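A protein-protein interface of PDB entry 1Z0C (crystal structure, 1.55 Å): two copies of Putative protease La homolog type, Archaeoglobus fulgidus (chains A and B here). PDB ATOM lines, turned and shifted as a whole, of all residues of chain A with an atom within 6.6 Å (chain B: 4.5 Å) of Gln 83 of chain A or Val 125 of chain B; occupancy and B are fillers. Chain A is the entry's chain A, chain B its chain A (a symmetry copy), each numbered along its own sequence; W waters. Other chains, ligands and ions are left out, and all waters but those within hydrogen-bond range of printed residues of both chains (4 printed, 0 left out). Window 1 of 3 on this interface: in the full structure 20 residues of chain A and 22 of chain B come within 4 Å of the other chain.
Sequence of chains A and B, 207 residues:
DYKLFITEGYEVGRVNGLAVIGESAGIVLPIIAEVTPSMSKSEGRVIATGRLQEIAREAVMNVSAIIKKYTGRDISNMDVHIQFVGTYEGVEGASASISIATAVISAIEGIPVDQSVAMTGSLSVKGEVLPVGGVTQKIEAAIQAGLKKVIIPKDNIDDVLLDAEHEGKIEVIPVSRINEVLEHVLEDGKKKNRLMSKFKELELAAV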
ATOM      1  N   GLY A  13     -22.483   6.810  10.930  1.00  0.00           N
ATOM      2  CA  GLY A  13     -22.974   8.200  10.982  1.00  0.00           C
ATOM      3  C   GLY A  13     -22.934   8.819  12.346  1.00  0.00           C
ATOM      4  O   GLY A  13     -23.414   9.959  12.529  1.00  0.00           O
ATOM      5  N   PRO A  30     -22.324  13.937  21.313  1.00  0.00           N
ATOM      6  CA  PRO A  30     -22.505  13.005  20.183  1.00  0.00           C
ATOM      7  C   PRO A  30     -23.109  13.700  18.968  1.00  0.00           C
ATOM      8  O   PRO A  30     -24.048  14.542  19.115  1.00  0.00           O
ATOM      9  CB  PRO A  30     -23.454  11.924  20.719  1.00  0.00           C
ATOM     10  CG  PRO A  30     -23.556  12.179  22.197  1.00  0.00           C
ATOM     11  CD  PRO A  30     -23.241  13.615  22.438  1.00  0.00           C
ATOM     12  N   ILE A  31     -22.540  13.371  17.839  1.00  0.00           N
ATOM     13  CA  ILE A  31     -22.994  13.932  16.554  1.00  0.00           C
ATOM     14  C   ILE A  31     -23.641  12.793  15.787  1.00  0.00           C
ATOM     15  O   ILE A  31     -23.109  11.667  15.793  1.00  0.00           O
ATOM     16  CB  ILE A  31     -21.772  14.406  15.688  1.00  0.00           C
ATOM     17  CG1 ILE A  31     -20.881  15.399  16.435  1.00  0.00           C
ATOM     18  CG2 ILE A  31     -22.305  15.029  14.381  1.00  0.00           C
ATOM     19  CD1 ILE A  31     -21.650  16.600  16.776  1.00  0.00           C
ATOM     20  N   ILE A  32     -24.776  13.019  15.071  1.00  0.00           N
ATOM     21  CA  ILE A  32     -25.263  12.036  14.118  1.00  0.00           C
ATOM     22  C   ILE A  32     -25.465  12.773  12.784  1.00  0.00           C
ATOM     23  O   ILE A  32     -25.898  13.954  12.770  1.00  0.00           O
ATOM     24  CB  ILE A  32     -26.592  11.416  14.546  1.00  0.00           C
ATOM     25  CG1 ILE A  32     -26.466  10.930  16.019  1.00  0.00           C
ATOM     26  CG2 ILE A  32     -27.031  10.261  13.593  1.00  0.00           C
ATOM     27  CD1 ILE A  32     -27.792  10.474  16.632  1.00  0.00           C
ATOM     28  N   ALA A  33     -25.004  12.133  11.720  1.00  0.00           N
ATOM     29  CA  ALA A  33     -25.158  12.675  10.368  1.00  0.00           C
ATOM     30  C   ALA A  33     -25.930  11.748   9.463  1.00  0.00           C
ATOM     31  O   ALA A  33     -25.800  10.513   9.580  1.00  0.00           O
ATOM     32  CB  ALA A  33     -23.757  12.932   9.791  1.00  0.00           C
ATOM     33  N   GLU A  34     -26.668  12.354   8.514  1.00  0.00           N
ATOM     34  CA  GLU A  34     -27.340  11.592   7.464  1.00  0.00           C
ATOM     35  C   GLU A  34     -27.157  12.400   6.192  1.00  0.00           C
ATOM     36  O   GLU A  34     -27.139  13.617   6.228  1.00  0.00           O
ATOM     37  CB  GLU A  34     -28.834  11.391   7.752  1.00  0.00           C
ATOM     38  CG  GLU A  34     -29.548  10.488   6.746  1.00  0.00           C
ATOM     39  CD  GLU A  34     -28.820   9.146   6.491  1.00  0.00           C
ATOM     40  OE1 GLU A  34     -27.743   9.058   5.870  1.00  0.00           O
ATOM     41  OE2 GLU A  34     -29.334   8.145   6.975  1.00  0.00           O
ATOM     42  N   ILE A  47     -28.181  20.926   6.499  1.00  0.00           N
ATOM     43  CA  ILE A  47     -29.297  21.174   7.379  1.00  0.00           C
ATOM     44  C   ILE A  47     -28.898  20.917   8.828  1.00  0.00           C
ATOM     45  O   ILE A  47     -28.499  19.830   9.172  1.00  0.00           O
ATOM     46  CB  ILE A  47     -30.478  20.350   6.957  1.00  0.00           C
ATOM     47  CG1 ILE A  47     -30.898  20.791   5.541  1.00  0.00           C
ATOM     48  CG2 ILE A  47     -31.592  20.575   7.930  1.00  0.00           C
ATOM     49  CD1 ILE A  47     -31.636  19.765   4.757  1.00  0.00           C
ATOM     50  N   ALA A  48     -28.958  21.959   9.648  1.00  0.00           N
ATOM     51  CA  ALA A  48     -28.562  21.951  11.040  1.00  0.00           C
ATOM     52  C   ALA A  48     -29.447  23.003  11.734  1.00  0.00           C
ATOM     53  O   ALA A  48     -29.782  24.030  11.147  1.00  0.00           O
ATOM     54  CB  ALA A  48     -27.065  22.311  11.173  1.00  0.00           C
ATOM     55  N   HIS A  81     -27.488  16.288   6.741  1.00  0.00           N
ATOM     56  CA  HIS A  81     -28.147  16.627   7.993  1.00  0.00           C
ATOM     57  C   HIS A  81     -27.242  16.386   9.182  1.00  0.00           C
ATOM     58  O   HIS A  81     -26.741  15.267   9.291  1.00  0.00           O
ATOM     59  CB  HIS A  81     -29.407  15.769   8.217  1.00  0.00           C
ATOM     60  CG  HIS A  81     -30.513  16.043   7.255  1.00  0.00           C
ATOM     61  ND1 HIS A  81     -31.681  16.683   7.610  1.00  0.00           N
ATOM     62  CD2 HIS A  81     -30.608  15.765   5.941  1.00  0.00           C
ATOM     63  CE1 HIS A  81     -32.462  16.782   6.540  1.00  0.00           C
ATOM     64  NE2 HIS A  81     -31.843  16.216   5.518  1.00  0.00           N
ATOM     65  N   ILE A  82     -27.059  17.375  10.039  1.00  0.00           N
ATOM     66  CA  ILE A  82     -26.193  17.254  11.232  1.00  0.00           C
ATOM     67  C   ILE A  82     -27.037  17.437  12.451  1.00  0.00           C
ATOM     68  O   ILE A  82     -27.703  18.490  12.622  1.00  0.00           O
ATOM     69  CB  ILE A  82     -25.061  18.321  11.242  1.00  0.00           C
ATOM     70  CG1 ILE A  82     -24.212  18.203   9.966  1.00  0.00           C
ATOM     71  CG2 ILE A  82     -24.197  18.147  12.485  1.00  0.00           C
ATOM     72  CD1 ILE A  82     -23.530  16.789   9.720  1.00  0.00           C
ATOM     73  N   GLN A  83     -27.000  16.429  13.311  1.00  0.00           N
ATOM     74  CA  GLN A  83     -27.714  16.488  14.579  1.00  0.00           C
ATOM     75  C   GLN A  83     -26.744  16.424  15.740  1.00  0.00           C
ATOM     76  O   GLN A  83     -25.832  15.636  15.701  1.00  0.00           O
ATOM     77  CB  GLN A  83     -28.611  15.279  14.687  1.00  0.00           C
ATOM     78  CG  GLN A  83     -29.330  15.075  16.007  1.00  0.00           C
ATOM     79  CD  GLN A  83     -30.322  13.948  15.938  1.00  0.00           C
ATOM     80  OE1 GLN A  83     -30.263  13.074  15.073  1.00  0.00           O
ATOM     81  NE2 GLN A  83     -31.336  14.009  16.864  1.00  0.00           N
ATOM     82  N   PHE A  84     -26.942  17.284  16.744  1.00  0.00           N
ATOM     83  CA  PHE A  84     -26.169  17.205  17.976  1.00  0.00           C
ATOM     84  C   PHE A  84     -27.099  16.613  18.982  1.00  0.00           C
ATOM     85  O   PHE A  84     -28.228  17.090  19.148  1.00  0.00           O
ATOM     86  CB  PHE A  84     -25.742  18.617  18.446  1.00  0.00           C
ATOM     87  CG  PHE A  84     -24.857  19.356  17.460  1.00  0.00           C
ATOM     88  CD1 PHE A  84     -23.480  19.247  17.487  1.00  0.00           C
ATOM     89  CD2 PHE A  84     -25.422  20.092  16.454  1.00  0.00           C
ATOM     90  CE1 PHE A  84     -22.696  19.905  16.559  1.00  0.00           C
ATOM     91  CE2 PHE A  84     -24.640  20.759  15.517  1.00  0.00           C
ATOM     92  CZ  PHE A  84     -23.270  20.680  15.601  1.00  0.00           C
ATOM     93  N   VAL A  85     -26.651  15.555  19.649  1.00  0.00           N
ATOM     94  CA  VAL A  85     -27.486  14.902  20.631  1.00  0.00           C
ATOM     95  C   VAL A  85     -27.286  15.538  22.011  1.00  0.00           C
ATOM     96  O   VAL A  85     -26.153  15.672  22.483  1.00  0.00           O
ATOM     97  CB  VAL A  85     -27.248  13.380  20.669  1.00  0.00           C
ATOM     98  CG1 VAL A  85     -28.384  12.717  21.343  1.00  0.00           C
ATOM     99  CG2 VAL A  85     -27.122  12.815  19.282  1.00  0.00           C
ATOM    100  N   ASN B  62     -35.151  16.760  11.195  1.00  0.00           N
ATOM    101  CA  ASN B  62     -34.692  15.356  11.297  1.00  0.00           C
ATOM    102  C   ASN B  62     -35.604  14.391  10.584  1.00  0.00           C
ATOM    103  O   ASN B  62     -35.177  13.425   9.921  1.00  0.00           O
ATOM    104  CB  ASN B  62     -34.573  14.926  12.768  1.00  0.00           C
ATOM    105  CG  ASN B  62     -33.448  15.595  13.482  1.00  0.00           C
ATOM    106  OD1 ASN B  62     -32.753  16.487  12.959  1.00  0.00           O
ATOM    107  ND2 ASN B  62     -33.297  15.205  14.733  1.00  0.00           N
ATOM    108  N   ALA B  65     -35.032  14.237   6.840  1.00  0.00           N
ATOM    109  CA  ALA B  65     -34.018  13.369   6.295  1.00  0.00           C
ATOM    110  C   ALA B  65     -34.579  11.988   5.956  1.00  0.00           C
ATOM    111  O   ALA B  65     -34.252  11.403   4.922  1.00  0.00           O
ATOM    112  CB  ALA B  65     -32.894  13.248   7.311  1.00  0.00           C
ATOM    113  N   ILE B  66     -35.359  11.458   6.890  1.00  0.00           N
ATOM    114  CA  ILE B  66     -35.920  10.121   6.758  1.00  0.00           C
ATOM    115  C   ILE B  66     -36.990  10.094   5.659  1.00  0.00           C
ATOM    116  O   ILE B  66     -37.058   9.114   4.877  1.00  0.00           O
ATOM    117  CB  ILE B  66     -36.547   9.676   8.115  1.00  0.00           C
ATOM    118  CG1 ILE B  66     -35.457   9.495   9.200  1.00  0.00           C
ATOM    119  CG2 ILE B  66     -37.235   8.333   7.936  1.00  0.00           C
ATOM    120  CD1 ILE B  66     -35.972   9.773  10.618  1.00  0.00           C
ATOM    121  N   ALA B  96     -36.094  17.017  19.033  1.00  0.00           N
ATOM    122  CA  ALA B  96     -36.414  16.253  17.815  1.00  0.00           C
ATOM    123  C   ALA B  96     -37.524  15.263  18.161  1.00  0.00           C
ATOM    124  O   ALA B  96     -37.416  14.090  17.874  1.00  0.00           O
ATOM    125  CB  ALA B  96     -35.185  15.490  17.265  1.00  0.00           C
ATOM    126  N   LEU B 123     -36.017  11.738  17.998  1.00  0.00           N
ATOM    127  CA  LEU B 123     -35.779  11.089  16.719  1.00  0.00           C
ATOM    128  C   LEU B 123     -34.380  11.421  16.216  1.00  0.00           C
ATOM    129  O   LEU B 123     -34.022  12.605  16.134  1.00  0.00           O
ATOM    130  CB  LEU B 123     -36.839  11.560  15.688  1.00  0.00           C
ATOM    131  CG  LEU B 123     -36.555  11.027  14.263  1.00  0.00           C
ATOM    132  CD1 LEU B 123     -36.843   9.537  14.257  1.00  0.00           C
ATOM    133  CD2 LEU B 123     -37.502  11.694  13.259  1.00  0.00           C
ATOM    134  N   SER B 124     -33.607  10.389  15.881  1.00  0.00           N
ATOM    135  CA  SER B 124     -32.377  10.660  15.213  1.00  0.00           C
ATOM    136  C   SER B 124     -32.585  10.808  13.710  1.00  0.00           C
ATOM    137  O   SER B 124     -33.568  10.287  13.163  1.00  0.00           O
ATOM    138  CB  SER B 124     -31.300   9.601  15.522  1.00  0.00           C
ATOM    139  OG  SER B 124     -31.168   8.625  14.519  1.00  0.00           O
ATOM    140  N   VAL B 125     -31.655  11.493  13.072  1.00  0.00           N
ATOM    141  CA  VAL B 125     -31.706  11.710  11.612  1.00  0.00           C
ATOM    142  C   VAL B 125     -31.566  10.407  10.864  1.00  0.00           C
ATOM    143  O   VAL B 125     -31.878  10.334   9.632  1.00  0.00           O
ATOM    144  CB  VAL B 125     -30.672  12.733  11.094  1.00  0.00           C
ATOM    145  CG1 VAL B 125     -30.989  14.098  11.575  1.00  0.00           C
ATOM    146  CG2 VAL B 125     -29.225  12.364  11.542  1.00  0.00           C
ATOM    147  N   LYS B 126     -31.154   9.382  11.571  1.00  0.00           N
ATOM    148  CA  LYS B 126     -31.024   8.044  11.016  1.00  0.00           C
ATOM    149  C   LYS B 126     -32.313   7.231  11.213  1.00  0.00           C
ATOM    150  O   LYS B 126     -32.449   6.112  10.675  1.00  0.00           O
ATOM    151  CB  LYS B 126     -29.805   7.321  11.609  1.00  0.00           C
ATOM    152  CG  LYS B 126     -28.529   7.916  11.163  1.00  0.00           C
ATOM    153  CD  LYS B 126     -27.370   7.115  11.694  1.00  0.00           C
ATOM    154  CE  LYS B 126     -27.602   5.642  11.615  1.00  0.00           C
ATOM    155  NZ  LYS B 126     -26.810   4.928  12.705  1.00  0.00           N
ATOM    156  N   GLY B 127     -33.293   7.779  11.936  1.00  0.00           N
ATOM    157  CA  GLY B 127     -34.524   7.025  12.186  1.00  0.00           C
ATOM    158  C   GLY B 127     -34.604   6.289  13.539  1.00  0.00           C
ATOM    159  O   GLY B 127     -35.582   5.638  13.836  1.00  0.00           O
HETATM  160  O   HOH W   1     -32.254   8.456   7.674  1.00  0.00           O
HETATM  161  O   HOH W   2     -30.775  17.887  14.096  1.00  0.00           O
HETATM  162  O   HOH W   3     -31.204   5.574   8.207  1.00  0.00           O
HETATM  163  O   HOH W   4     -31.690  17.532  10.364  1.00  0.00           O
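No position is printed for both chains.
The backbone NH (N) of Gln 83 of chain A sits at hydrogen-bond distance from the backbone carbonyl oxygen (O) of Ile 32 of chain A.
The backbone NH (N) of His 81 of chain A lies within hydrogen-bond range of the backbone carbonyl oxygen (O) of Glu 34 of chain A, 2.7 Å away.
ND2 of Asn 62 of chain B lies within hydrogen-bond range of O of Leu 123 of chain B, 3.0 Å away.
The backbone carbonyl oxygen of Ala 96 of chain B sits at hydrogen-bond distance from the backbone NH of Leu 123 of chain B, 2.7 Å away.
The side-chain hydroxyl (OG) of Ser 124 of chain B sits close to the backbone NH (N) of Lys 126 of chain B (3.0 Å).
The side-chain hydroxyl of Ser 124 of chain B is in hydrogen-bond range of the backbone NH of Gly 127 of chain B (3.5 Å).
Ile 47 of chain A touches none of the printed residues of chain B.
Printed residues of chain B within 4 Å of His 81 of chain A: Ala 65.
Gln 83 of chain A touches just these residues of chain B: Asn 62 (3.1 Å), Leu 123 (3.1 Å), Ser 124 (3.2 Å) and Val 125 (2.9 Å).
Val 125 of chain B touches just these residues of chain A: Ile 32 (3.7 Å), Ala 33 (3.9 Å), Glu 34 (3.7 Å) and Gln 83 (2.9 Å).
Of the printed residues of chain A, Lys 126 of chain B touches Ile 32 (3.7 Å).
Hydrophobic or aromatic side chains of chain B within 4 Å of the printed part of chain A: Ala 65 and Val 125.
Among the printed residues, no Asp or Glu carboxylate lies within 4 Å of a Lys or Arg side-chain nitrogen of the other chain.
Water W2 lies within hydrogen-bond range of the side-chain amide oxygen of Asn 62 of chain B (2.7 Å) and the backbone carbonyl oxygen of Ile 82 of chain A (3.5 Å).
Water W1 bridges O of Val 125 of chain B and OE2 of Glu 34 of chain A.
Water W3 lies within hydrogen-bond range of the backbone carbonyl oxygen (O) of Lys 126 of chain B (2.8 Å) and the side-chain carboxylate (OE2) of Glu 34 of chain A (3.4 Å).
Water W4 bridges a ring nitrogen (ND1) of His 81 of chain A (2.9 Å) and the side-chain amide oxygen (OD1) of Asn 62 of chain B (3.0 Å).
The side-chain amide nitrogen (NE2) of Gln 83 of chain A sits close to the side-chain amide nitrogen (ND2) of Asn 62 of chain B (3.1 Å).
O of Leu 123 of chain B lies within hydrogen-bond range of NE2 of Gln 83 of chain A.
The side-chain amide oxygen (OE1) of Gln 83 of chain A sits at hydrogen-bond distance from the backbone NH (N) of Val 125 of chain B, 2.9 Å away.
Among the printed residues, merely in contact across the chains: Gln 83 of chain A with Ser 124 of chain B (3.2 Å), His 81 of chain A with Ala 65 of chain B (3.6 Å), Ile 32 of chain A with Val 125 of chain B (3.7 Å), Ile 32 of chain A with Lys 126 of chain B (3.7 Å), Glu 34 of chain A with Val 125 of chain B (3.7 Å), Ile 32 of chain A with Ser 124 of chain B (3.8 Å) and Ala 33 of chain A with Val 125 of chain B (3.9 Å).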
